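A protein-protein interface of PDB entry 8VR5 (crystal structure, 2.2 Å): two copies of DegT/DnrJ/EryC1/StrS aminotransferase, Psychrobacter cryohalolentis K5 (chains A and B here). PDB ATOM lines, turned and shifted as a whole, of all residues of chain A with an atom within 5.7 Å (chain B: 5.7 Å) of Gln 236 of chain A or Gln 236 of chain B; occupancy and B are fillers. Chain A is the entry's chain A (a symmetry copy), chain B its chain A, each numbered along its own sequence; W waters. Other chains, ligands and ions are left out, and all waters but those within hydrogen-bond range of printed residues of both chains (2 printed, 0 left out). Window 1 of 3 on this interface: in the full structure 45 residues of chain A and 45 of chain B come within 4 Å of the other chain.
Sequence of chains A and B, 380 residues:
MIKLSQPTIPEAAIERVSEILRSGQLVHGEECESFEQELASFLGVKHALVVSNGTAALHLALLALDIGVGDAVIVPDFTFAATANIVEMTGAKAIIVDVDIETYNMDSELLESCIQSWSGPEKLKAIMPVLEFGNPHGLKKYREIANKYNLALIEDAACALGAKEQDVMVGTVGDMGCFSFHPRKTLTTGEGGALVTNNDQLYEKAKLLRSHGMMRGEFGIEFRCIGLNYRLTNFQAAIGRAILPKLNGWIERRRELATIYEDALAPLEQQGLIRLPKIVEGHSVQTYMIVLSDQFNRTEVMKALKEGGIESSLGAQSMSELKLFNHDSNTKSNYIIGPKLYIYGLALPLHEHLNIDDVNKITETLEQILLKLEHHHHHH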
ATOM      1  N   VAL A  17       6.065  31.510  11.729  1.00  0.00           N
ATOM      2  CA  VAL A  17       6.728  30.352  11.128  1.00  0.00           C
ATOM      3  C   VAL A  17       5.711  29.458  10.406  1.00  0.00           C
ATOM      4  O   VAL A  17       5.927  29.043   9.252  1.00  0.00           O
ATOM      5  CB  VAL A  17       7.549  29.570  12.178  1.00  0.00           C
ATOM      6  CG1 VAL A  17       8.057  28.215  11.680  1.00  0.00           C
ATOM      7  CG2 VAL A  17       8.717  30.418  12.687  1.00  0.00           C
ATOM      8  N   PHE A  35      15.339  41.456   9.286  1.00  0.00           N
ATOM      9  CA  PHE A  35      16.038  41.091  10.505  1.00  0.00           C
ATOM     10  C   PHE A  35      17.398  41.771  10.492  1.00  0.00           C
ATOM     11  O   PHE A  35      17.815  42.320  11.496  1.00  0.00           O
ATOM     12  CB  PHE A  35      16.162  39.573  10.660  1.00  0.00           C
ATOM     13  CG  PHE A  35      16.694  39.076  11.983  1.00  0.00           C
ATOM     14  CD1 PHE A  35      16.613  39.832  13.131  1.00  0.00           C
ATOM     15  CD2 PHE A  35      17.257  37.810  12.081  1.00  0.00           C
ATOM     16  CE1 PHE A  35      17.109  39.348  14.335  1.00  0.00           C
ATOM     17  CE2 PHE A  35      17.736  37.321  13.283  1.00  0.00           C
ATOM     18  CZ  PHE A  35      17.665  38.092  14.416  1.00  0.00           C
ATOM     19  N   SER A  52      24.052  31.051   9.194  1.00  0.00           N
ATOM     20  CA  SER A  52      23.580  29.772   9.699  1.00  0.00           C
ATOM     21  C   SER A  52      23.801  29.606  11.201  1.00  0.00           C
ATOM     22  O   SER A  52      23.010  28.946  11.868  1.00  0.00           O
ATOM     23  CB  SER A  52      24.263  28.678   8.931  1.00  0.00           C
ATOM     24  OG  SER A  52      24.075  28.870   7.520  1.00  0.00           O
ATOM     25  N   THR A 189      17.463  31.390  17.365  1.00  0.00           N
ATOM     26  CA  THR A 189      16.707  31.027  16.178  1.00  0.00           C
ATOM     27  C   THR A 189      16.916  29.532  15.949  1.00  0.00           C
ATOM     28  O   THR A 189      16.784  28.987  14.843  1.00  0.00           O
ATOM     29  CB  THR A 189      17.117  31.815  14.930  1.00  0.00           C
ATOM     30  OG1 THR A 189      18.498  31.567  14.659  1.00  0.00           O
ATOM     31  CG2 THR A 189      16.935  33.302  15.080  1.00  0.00           C
ATOM     32  N   GLY A 190      17.195  28.856  17.049  1.00  0.00           N
ATOM     33  CA  GLY A 190      17.521  27.454  16.999  1.00  0.00           C
ATOM     34  C   GLY A 190      18.987  27.223  16.658  1.00  0.00           C
ATOM     35  O   GLY A 190      19.714  26.698  17.489  1.00  0.00           O
ATOM     36  N   GLU A 191      19.371  27.532  15.410  1.00  0.00           N
ATOM     37  CA  GLU A 191      20.746  27.793  15.039  1.00  0.00           C
ATOM     38  C   GLU A 191      20.693  29.104  14.282  1.00  0.00           C
ATOM     39  O   GLU A 191      19.703  29.368  13.591  1.00  0.00           O
ATOM     40  CB  GLU A 191      21.334  26.721  14.107  1.00  0.00           C
ATOM     41  CG  GLU A 191      21.528  25.344  14.743  1.00  0.00           C
ATOM     42  CD  GLU A 191      22.805  25.113  15.539  1.00  0.00           C
ATOM     43  OE1 GLU A 191      23.634  26.053  15.680  1.00  0.00           O
ATOM     44  OE2 GLU A 191      23.012  23.957  15.954  1.00  0.00           O
ATOM     45  N   GLY A 192      21.721  29.930  14.436  1.00  0.00           N
ATOM     46  CA  GLY A 192      21.737  31.200  13.745  1.00  0.00           C
ATOM     47  C   GLY A 192      22.826  32.110  14.280  1.00  0.00           C
ATOM     48  O   GLY A 192      23.500  31.773  15.247  1.00  0.00           O
ATOM     49  N   LEU A 232      20.731  31.807   6.389  1.00  0.00           N
ATOM     50  CA  LEU A 232      19.678  31.517   7.327  1.00  0.00           C
ATOM     51  C   LEU A 232      18.350  31.448   6.583  1.00  0.00           C
ATOM     52  O   LEU A 232      18.127  32.163   5.612  1.00  0.00           O
ATOM     53  CB  LEU A 232      19.685  32.599   8.410  1.00  0.00           C
ATOM     54  CG  LEU A 232      18.815  32.311   9.615  1.00  0.00           C
ATOM     55  CD1 LEU A 232      19.353  31.160  10.458  1.00  0.00           C
ATOM     56  CD2 LEU A 232      18.635  33.552  10.464  1.00  0.00           C
ATOM     57  N   THR A 233      17.449  30.612   7.076  1.00  0.00           N
ATOM     58  CA  THR A 233      16.111  30.530   6.522  1.00  0.00           C
ATOM     59  C   THR A 233      15.234  31.679   7.008  1.00  0.00           C
ATOM     60  O   THR A 233      15.383  32.205   8.117  1.00  0.00           O
ATOM     61  CB  THR A 233      15.362  29.264   6.917  1.00  0.00           C
ATOM     62  OG1 THR A 233      15.009  29.398   8.292  1.00  0.00           O
ATOM     63  CG2 THR A 233      16.172  28.006   6.703  1.00  0.00           C
ATOM     64  N   ASN A 234      14.299  32.028   6.123  1.00  0.00           N
ATOM     65  CA  ASN A 234      13.342  33.086   6.310  1.00  0.00           C
ATOM     66  C   ASN A 234      12.525  32.862   7.585  1.00  0.00           C
ATOM     67  O   ASN A 234      12.197  33.818   8.279  1.00  0.00           O
ATOM     68  CB  ASN A 234      12.484  33.179   5.048  1.00  0.00           C
ATOM     69  CG  ASN A 234      11.892  34.553   4.804  1.00  0.00           C
ATOM     70  OD1 ASN A 234      12.593  35.577   4.878  1.00  0.00           O
ATOM     71  ND2 ASN A 234      10.601  34.575   4.465  1.00  0.00           N
ATOM     72  N   PHE A 235      12.192  31.614   7.916  1.00  0.00           N
ATOM     73  CA  PHE A 235      11.405  31.365   9.103  1.00  0.00           C
ATOM     74  C   PHE A 235      12.232  31.468  10.377  1.00  0.00           C
ATOM     75  O   PHE A 235      11.708  31.837  11.427  1.00  0.00           O
ATOM     76  CB  PHE A 235      10.668  30.026   9.060  1.00  0.00           C
ATOM     77  CG  PHE A 235      11.412  28.780   8.659  1.00  0.00           C
ATOM     78  CD1 PHE A 235      11.515  28.424   7.322  1.00  0.00           C
ATOM     79  CD2 PHE A 235      11.878  27.901   9.613  1.00  0.00           C
ATOM     80  CE1 PHE A 235      12.158  27.257   6.948  1.00  0.00           C
ATOM     81  CE2 PHE A 235      12.517  26.736   9.236  1.00  0.00           C
ATOM     82  CZ  PHE A 235      12.647  26.411   7.906  1.00  0.00           C
ATOM     83  N   GLN A 236      13.500  31.063  10.313  1.00  0.00           N
ATOM     84  CA  GLN A 236      14.380  31.314  11.439  1.00  0.00           C
ATOM     85  C   GLN A 236      14.513  32.828  11.668  1.00  0.00           C
ATOM     86  O   GLN A 236      14.548  33.279  12.806  1.00  0.00           O
ATOM     87  CB  GLN A 236      15.745  30.672  11.214  1.00  0.00           C
ATOM     88  CG  GLN A 236      15.740  29.184  11.494  1.00  0.00           C
ATOM     89  CD  GLN A 236      16.935  28.522  10.860  1.00  0.00           C
ATOM     90  OE1 GLN A 236      17.026  28.412   9.628  1.00  0.00           O
ATOM     91  NE2 GLN A 236      17.896  28.156  11.691  1.00  0.00           N
ATOM     92  N   ALA A 237      14.585  33.610  10.593  1.00  0.00           N
ATOM     93  CA  ALA A 237      14.818  35.030  10.746  1.00  0.00           C
ATOM     94  C   ALA A 237      13.621  35.640  11.465  1.00  0.00           C
ATOM     95  O   ALA A 237      13.793  36.439  12.381  1.00  0.00           O
ATOM     96  CB  ALA A 237      15.072  35.680   9.418  1.00  0.00           C
ATOM     97  N   ALA A 238      12.434  35.134  11.115  1.00  0.00           N
ATOM     98  CA  ALA A 238      11.184  35.601  11.690  1.00  0.00           C
ATOM     99  C   ALA A 238      11.199  35.363  13.185  1.00  0.00           C
ATOM    100  O   ALA A 238      10.649  36.169  13.917  1.00  0.00           O
ATOM    101  CB  ALA A 238       9.993  34.896  11.072  1.00  0.00           C
ATOM    102  N   ILE A 239      11.765  34.229  13.603  1.00  0.00           N
ATOM    103  CA  ILE A 239      11.845  33.923  15.012  1.00  0.00           C
ATOM    104  C   ILE A 239      12.651  35.019  15.672  1.00  0.00           C
ATOM    105  O   ILE A 239      12.264  35.543  16.712  1.00  0.00           O
ATOM    106  CB  ILE A 239      12.445  32.543  15.296  1.00  0.00           C
ATOM    107  CG1 ILE A 239      11.523  31.417  14.826  1.00  0.00           C
ATOM    108  CG2 ILE A 239      12.787  32.419  16.762  1.00  0.00           C
ATOM    109  CD1 ILE A 239      12.128  30.039  14.909  1.00  0.00           C
ATOM    110  N   GLY A 240      13.770  35.370  15.033  1.00  0.00           N
ATOM    111  CA  GLY A 240      14.704  36.270  15.668  1.00  0.00           C
ATOM    112  C   GLY A 240      14.119  37.670  15.752  1.00  0.00           C
ATOM    113  O   GLY A 240      14.400  38.387  16.703  1.00  0.00           O
ATOM    114  N   ARG A 241      13.349  38.048  14.721  1.00  0.00           N
ATOM    115  CA  ARG A 241      12.795  39.385  14.641  1.00  0.00           C
ATOM    116  C   ARG A 241      11.780  39.595  15.748  1.00  0.00           C
ATOM    117  O   ARG A 241      11.541  40.728  16.138  1.00  0.00           O
ATOM    118  CB  ARG A 241      12.026  39.635  13.356  1.00  0.00           C
ATOM    119  CG  ARG A 241      12.850  39.451  12.107  1.00  0.00           C
ATOM    120  CD  ARG A 241      12.018  39.801  10.897  1.00  0.00           C
ATOM    121  NE  ARG A 241      11.500  41.160  10.952  1.00  0.00           N
ATOM    122  CZ  ARG A 241      10.450  41.621  10.252  1.00  0.00           C
ATOM    123  NH1 ARG A 241      10.081  42.892  10.357  1.00  0.00           N
ATOM    124  NH2 ARG A 241       9.813  40.839   9.398  1.00  0.00           N
ATOM    125  N   VAL B  17       6.655  21.457  14.207  1.00  0.00           N
ATOM    126  CA  VAL B  17       7.545  22.604  14.391  1.00  0.00           C
ATOM    127  C   VAL B  17       7.038  23.509  15.522  1.00  0.00           C
ATOM    128  O   VAL B  17       7.807  23.917  16.411  1.00  0.00           O
ATOM    129  CB  VAL B  17       7.742  23.378  13.068  1.00  0.00           C
ATOM    130  CG1 VAL B  17       8.450  24.724  13.241  1.00  0.00           C
ATOM    131  CG2 VAL B  17       8.487  22.516  12.047  1.00  0.00           C
ATOM    132  N   PHE B  35      15.770  11.376  11.723  1.00  0.00           N
ATOM    133  CA  PHE B  35      15.771  11.735  10.316  1.00  0.00           C
ATOM    134  C   PHE B  35      16.946  11.037   9.650  1.00  0.00           C
ATOM    135  O   PHE B  35      16.797  10.486   8.574  1.00  0.00           O
ATOM    136  CB  PHE B  35      15.822  13.252  10.114  1.00  0.00           C
ATOM    137  CG  PHE B  35      15.628  13.747   8.701  1.00  0.00           C
ATOM    138  CD1 PHE B  35      14.973  12.996   7.749  1.00  0.00           C
ATOM    139  CD2 PHE B  35      16.084  15.005   8.330  1.00  0.00           C
ATOM    140  CE1 PHE B  35      14.808  13.477   6.457  1.00  0.00           C
ATOM    141  CE2 PHE B  35      15.904  15.492   7.048  1.00  0.00           C
ATOM    142  CZ  PHE B  35      15.266  14.726   6.104  1.00  0.00           C
ATOM    143  N   SER B  52      23.504  21.659   7.408  1.00  0.00           N
ATOM    144  CA  SER B  52      22.860  22.946   7.202  1.00  0.00           C
ATOM    145  C   SER B  52      22.303  23.115   5.790  1.00  0.00           C
ATOM    146  O   SER B  52      21.294  23.789   5.605  1.00  0.00           O
ATOM    147  CB  SER B  52      23.851  24.028   7.522  1.00  0.00           C
ATOM    148  OG  SER B  52      24.391  23.834   8.838  1.00  0.00           O
ATOM    149  N   THR B 189      13.709  21.441   3.627  1.00  0.00           N
ATOM    150  CA  THR B 189      13.653  21.810   5.031  1.00  0.00           C
ATOM    151  C   THR B 189      13.969  23.301   5.119  1.00  0.00           C
ATOM    152  O   THR B 189      14.414  23.844   6.141  1.00  0.00           O
ATOM    153  CB  THR B 189      14.620  21.012   5.910  1.00  0.00           C
ATOM    154  OG1 THR B 189      15.955  21.239   5.453  1.00  0.00           O
ATOM    155  CG2 THR B 189      14.368  19.528   5.876  1.00  0.00           C
ATOM    156  N   GLY B 190      13.670  23.977   4.026  1.00  0.00           N
ATOM    157  CA  GLY B 190      13.996  25.375   3.900  1.00  0.00           C
ATOM    158  C   GLY B 190      15.439  25.584   3.462  1.00  0.00           C
ATOM    159  O   GLY B 190      15.661  26.102   2.376  1.00  0.00           O
ATOM    160  N   GLU B 191      16.392  25.266   4.352  1.00  0.00           N
ATOM    161  CA  GLU B 191      17.764  24.984   3.987  1.00  0.00           C
ATOM    162  C   GLU B 191      18.078  23.671   4.674  1.00  0.00           C
ATOM    163  O   GLU B 191      17.563  23.418   5.768  1.00  0.00           O
ATOM    164  CB  GLU B 191      18.754  26.044   4.496  1.00  0.00           C
ATOM    165  CG  GLU B 191      18.623  27.420   3.843  1.00  0.00           C
ATOM    166  CD  GLU B 191      19.335  27.637   2.514  1.00  0.00           C
ATOM    167  OE1 GLU B 191      19.969  26.686   1.981  1.00  0.00           O
ATOM    168  OE2 GLU B 191      19.322  28.792   2.048  1.00  0.00           O
ATOM    169  N   GLY B 192      18.881  22.832   4.029  1.00  0.00           N
ATOM    170  CA  GLY B 192      19.223  21.559   4.625  1.00  0.00           C
ATOM    171  C   GLY B 192      19.886  20.636   3.620  1.00  0.00           C
ATOM    172  O   GLY B 192      19.990  20.968   2.444  1.00  0.00           O
ATOM    173  N   LEU B 232      22.020  20.938  11.501  1.00  0.00           N
ATOM    174  CA  LEU B 232      20.644  21.246  11.213  1.00  0.00           C
ATOM    175  C   LEU B 232      19.867  21.331  12.522  1.00  0.00           C
ATOM    176  O   LEU B 232      20.149  20.616  13.476  1.00  0.00           O
ATOM    177  CB  LEU B 232      20.093  20.169  10.276  1.00  0.00           C
ATOM    178  CG  LEU B 232      18.741  20.473   9.667  1.00  0.00           C
ATOM    179  CD1 LEU B 232      18.802  21.619   8.663  1.00  0.00           C
ATOM    180  CD2 LEU B 232      18.144  19.238   9.026  1.00  0.00           C
ATOM    181  N   THR B 233      18.851  22.182  12.541  1.00  0.00           N
ATOM    182  CA  THR B 233      17.971  22.279  13.690  1.00  0.00           C
ATOM    183  C   THR B 233      16.952  21.145  13.712  1.00  0.00           C
ATOM    184  O   THR B 233      16.520  20.621  12.679  1.00  0.00           O
ATOM    185  CB  THR B 233      17.142  23.557  13.718  1.00  0.00           C
ATOM    186  OG1 THR B 233      16.147  23.433  12.704  1.00  0.00           O
ATOM    187  CG2 THR B 233      17.968  24.803  13.494  1.00  0.00           C
ATOM    188  N   ASN B 234      16.580  20.805  14.947  1.00  0.00           N
ATOM    189  CA  ASN B 234      15.644  19.761  15.267  1.00  0.00           C
ATOM    190  C   ASN B 234      14.302  20.001  14.571  1.00  0.00           C
ATOM    191  O   ASN B 234      13.658  19.053  14.137  1.00  0.00           O
ATOM    192  CB  ASN B 234      15.530  19.676  16.789  1.00  0.00           C
ATOM    193  CG  ASN B 234      15.120  18.308  17.302  1.00  0.00           C
ATOM    194  OD1 ASN B 234      15.677  17.275  16.891  1.00  0.00           O
ATOM    195  ND2 ASN B 234      14.172  18.304  18.241  1.00  0.00           N
ATOM    196  N   PHE B 235      13.865  21.255  14.446  1.00  0.00           N
ATOM    197  CA  PHE B 235      12.594  21.519  13.811  1.00  0.00           C
ATOM    198  C   PHE B 235      12.671  21.410  12.294  1.00  0.00           C
ATOM    199  O   PHE B 235      11.688  21.051  11.648  1.00  0.00           O
ATOM    200  CB  PHE B 235      11.996  22.868  14.212  1.00  0.00           C
ATOM    201  CG  PHE B 235      12.857  24.102  14.182  1.00  0.00           C
ATOM    202  CD1 PHE B 235      13.620  24.451  15.288  1.00  0.00           C
ATOM    203  CD2 PHE B 235      12.796  24.978  13.120  1.00  0.00           C
ATOM    204  CE1 PHE B 235      14.379  25.608  15.286  1.00  0.00           C
ATOM    205  CE2 PHE B 235      13.554  26.133  13.123  1.00  0.00           C
ATOM    206  CZ  PHE B 235      14.336  26.451  14.208  1.00  0.00           C
ATOM    207  N   GLN B 236      13.807  21.797  11.714  1.00  0.00           N
ATOM    208  CA  GLN B 236      14.003  21.538  10.300  1.00  0.00           C
ATOM    209  C   GLN B 236      13.983  20.023  10.041  1.00  0.00           C
ATOM    210  O   GLN B 236      13.438  19.576   9.040  1.00  0.00           O
ATOM    211  CB  GLN B 236      15.306  22.160   9.810  1.00  0.00           C
ATOM    212  CG  GLN B 236      15.182  23.649   9.564  1.00  0.00           C
ATOM    213  CD  GLN B 236      16.543  24.292   9.514  1.00  0.00           C
ATOM    214  OE1 GLN B 236      17.240  24.397  10.534  1.00  0.00           O
ATOM    215  NE2 GLN B 236      16.965  24.648   8.312  1.00  0.00           N
ATOM    216  N   ALA B 237      14.572  19.236  10.939  1.00  0.00           N
ATOM    217  CA  ALA B 237      14.677  17.813  10.695  1.00  0.00           C
ATOM    218  C   ALA B 237      13.273  17.222  10.673  1.00  0.00           C
ATOM    219  O   ALA B 237      12.953  16.425   9.797  1.00  0.00           O
ATOM    220  CB  ALA B 237      15.552  17.155  11.720  1.00  0.00           C
ATOM    221  N   ALA B 238      12.426  17.743  11.568  1.00  0.00           N
ATOM    222  CA  ALA B 238      11.051  17.296  11.696  1.00  0.00           C
ATOM    223  C   ALA B 238      10.319  17.539  10.393  1.00  0.00           C
ATOM    224  O   ALA B 238       9.466  16.743  10.037  1.00  0.00           O
ATOM    225  CB  ALA B 238      10.338  18.015  12.824  1.00  0.00           C
ATOM    226  N   ILE B 239      10.616  18.667   9.743  1.00  0.00           N
ATOM    227  CA  ILE B 239       9.986  18.977   8.482  1.00  0.00           C
ATOM    228  C   ILE B 239      10.339  17.873   7.512  1.00  0.00           C
ATOM    229  O   ILE B 239       9.476  17.358   6.807  1.00  0.00           O
ATOM    230  CB  ILE B 239      10.382  20.350   7.931  1.00  0.00           C
ATOM    231  CG1 ILE B 239       9.834  21.487   8.795  1.00  0.00           C
ATOM    232  CG2 ILE B 239       9.948  20.474   6.491  1.00  0.00           C
ATOM    233  CD1 ILE B 239      10.335  22.856   8.416  1.00  0.00           C
ATOM    234  N   GLY B 240      11.622  17.504   7.507  1.00  0.00           N
ATOM    235  CA  GLY B 240      12.101  16.593   6.494  1.00  0.00           C
ATOM    236  C   GLY B 240      11.533  15.202   6.718  1.00  0.00           C
ATOM    237  O   GLY B 240      11.291  14.484   5.757  1.00  0.00           O
ATOM    238  N   ARG B 241      11.376  14.830   7.998  1.00  0.00           N
ATOM    239  CA  ARG B 241      10.918  13.501   8.349  1.00  0.00           C
ATOM    240  C   ARG B 241       9.483  13.309   7.898  1.00  0.00           C
ATOM    241  O   ARG B 241       9.065  12.181   7.684  1.00  0.00           O
ATOM    242  CB  ARG B 241      10.892  13.257   9.847  1.00  0.00           C
ATOM    243  CG  ARG B 241      12.232  13.425  10.516  1.00  0.00           C
ATOM    244  CD  ARG B 241      12.112  13.082  11.982  1.00  0.00           C
ATOM    245  NE  ARG B 241      11.617  11.731  12.197  1.00  0.00           N
ATOM    246  CZ  ARG B 241      11.051  11.281  13.331  1.00  0.00           C
ATOM    247  NH1 ARG B 241      10.662  10.017  13.429  1.00  0.00           N
ATOM    248  NH2 ARG B 241      10.938  12.069  14.385  1.00  0.00           N
HETATM  249  O   HOH W   1      17.925  30.707   3.201  1.00  0.00           O
HETATM  250  O   HOH W   2      21.199  22.066  15.660  1.00  0.00           O
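Val 17 of chain A touches its own counterpart, Val 17 of chain B. Thr 189 of chain A touches Phe 235 of chain B, and with the chains exchanged Phe 235 of chain A touches Thr 189 of chain B. Thr 233 of chain A touches Gln 236 of chain B, and with the chains exchanged Gln 236 of chain A touches Thr 233 of chain B. Gln 236 of chain B touches its own counterpart, Gln 236 of chain A. Positions printed for both chains: 17, 35, 52, 189, 190, 191, 192, 232, 233, 234, 235, 236, 237, 238, 239, 240 and 241.
The side-chain amide oxygen (OE1) of Gln 236 of chain B sits at hydrogen-bond distance from the side-chain hydroxyl (OG1) of Thr 233 of chain B, 2.6 Å away. The side-chain amide nitrogen of Gln 236 of chain A lies within hydrogen-bond range of the backbone carbonyl oxygen of Thr 189 of chain A, 3.4 Å away. O of Thr 189 of chain B sits at hydrogen-bond distance from NE2 of Gln 236 of chain B. The side-chain hydroxyl (OG1) of Thr 189 of chain A is in hydrogen-bond range of the backbone carbonyl oxygen (O) of Glu 191 of chain A, at 2.7 Å. The side-chain hydroxyl (OG1) of Thr 233 of chain A is in hydrogen-bond range of the side-chain amide oxygen (OE1) of Gln 236 of chain A, 2.6 Å away. O of Glu 191 of chain A sits at hydrogen-bond distance from NE2 of Gln 236 of chain A, at 2.9 Å.
Water W1 bridges the side-chain carboxylate (OE2) of Glu 191 of chain B (2.6 Å) and the backbone carbonyl oxygen (O) of Leu 232 of chain A (2.8 Å). Water W2 bridges the side-chain carboxylate of Glu 191 of chain A (2.6 Å) and the backbone carbonyl oxygen of Leu 232 of chain B (2.8 Å).
Val 17 of chain A touches Val 17 of chain B (CG1 to CG1, 3.8 Å). Thr 189 of chain A touches Phe 235 of chain B. Thr 233 of chain B touches Glu 191 of chain A (CG2 to N, 3.6 Å). Thr 233 of chain A touches Glu 191 of chain B. Gln 236 of chain B touches Thr 233 of chain A. CZ of Phe 235 of chain A touches O of Thr 189 of chain B (3.6 Å). Thr 233 of chain B touches Gln 236 of chain A (CG2 to NE2, 3.8 Å). Gln 236 of chain B touches Gln 236 of chain A.
Of the 17 printed residues of chain A, 6 touch a printed residue of chain B. Of the 17 printed residues of chain B, 6 touch a printed residue of chain A. Among the printed residues, 8 pairs touch across the chains. Among the printed residues, no Asp or Glu carboxylate lies within 4 Å of a Lys or Arg side-chain nitrogen of the other chain.
Printed residues of chain B within 4 Å of Phe 235 of chain A: Thr 189 (3.6 Å). Of the printed residues of chain A, Val 17 of chain B touches Val 17. Of the printed residues of chain A, Gln 236 of chain B touches Thr 233 and Gln 236. The nearest printed residue of chain B that does not touch Gln 236 of chain A is Phe 235 of chain B (4.1 Å). The nearest printed residue of chain A that does not touch Val 17 of chain B is Phe 235 of chain A (5.9 Å).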
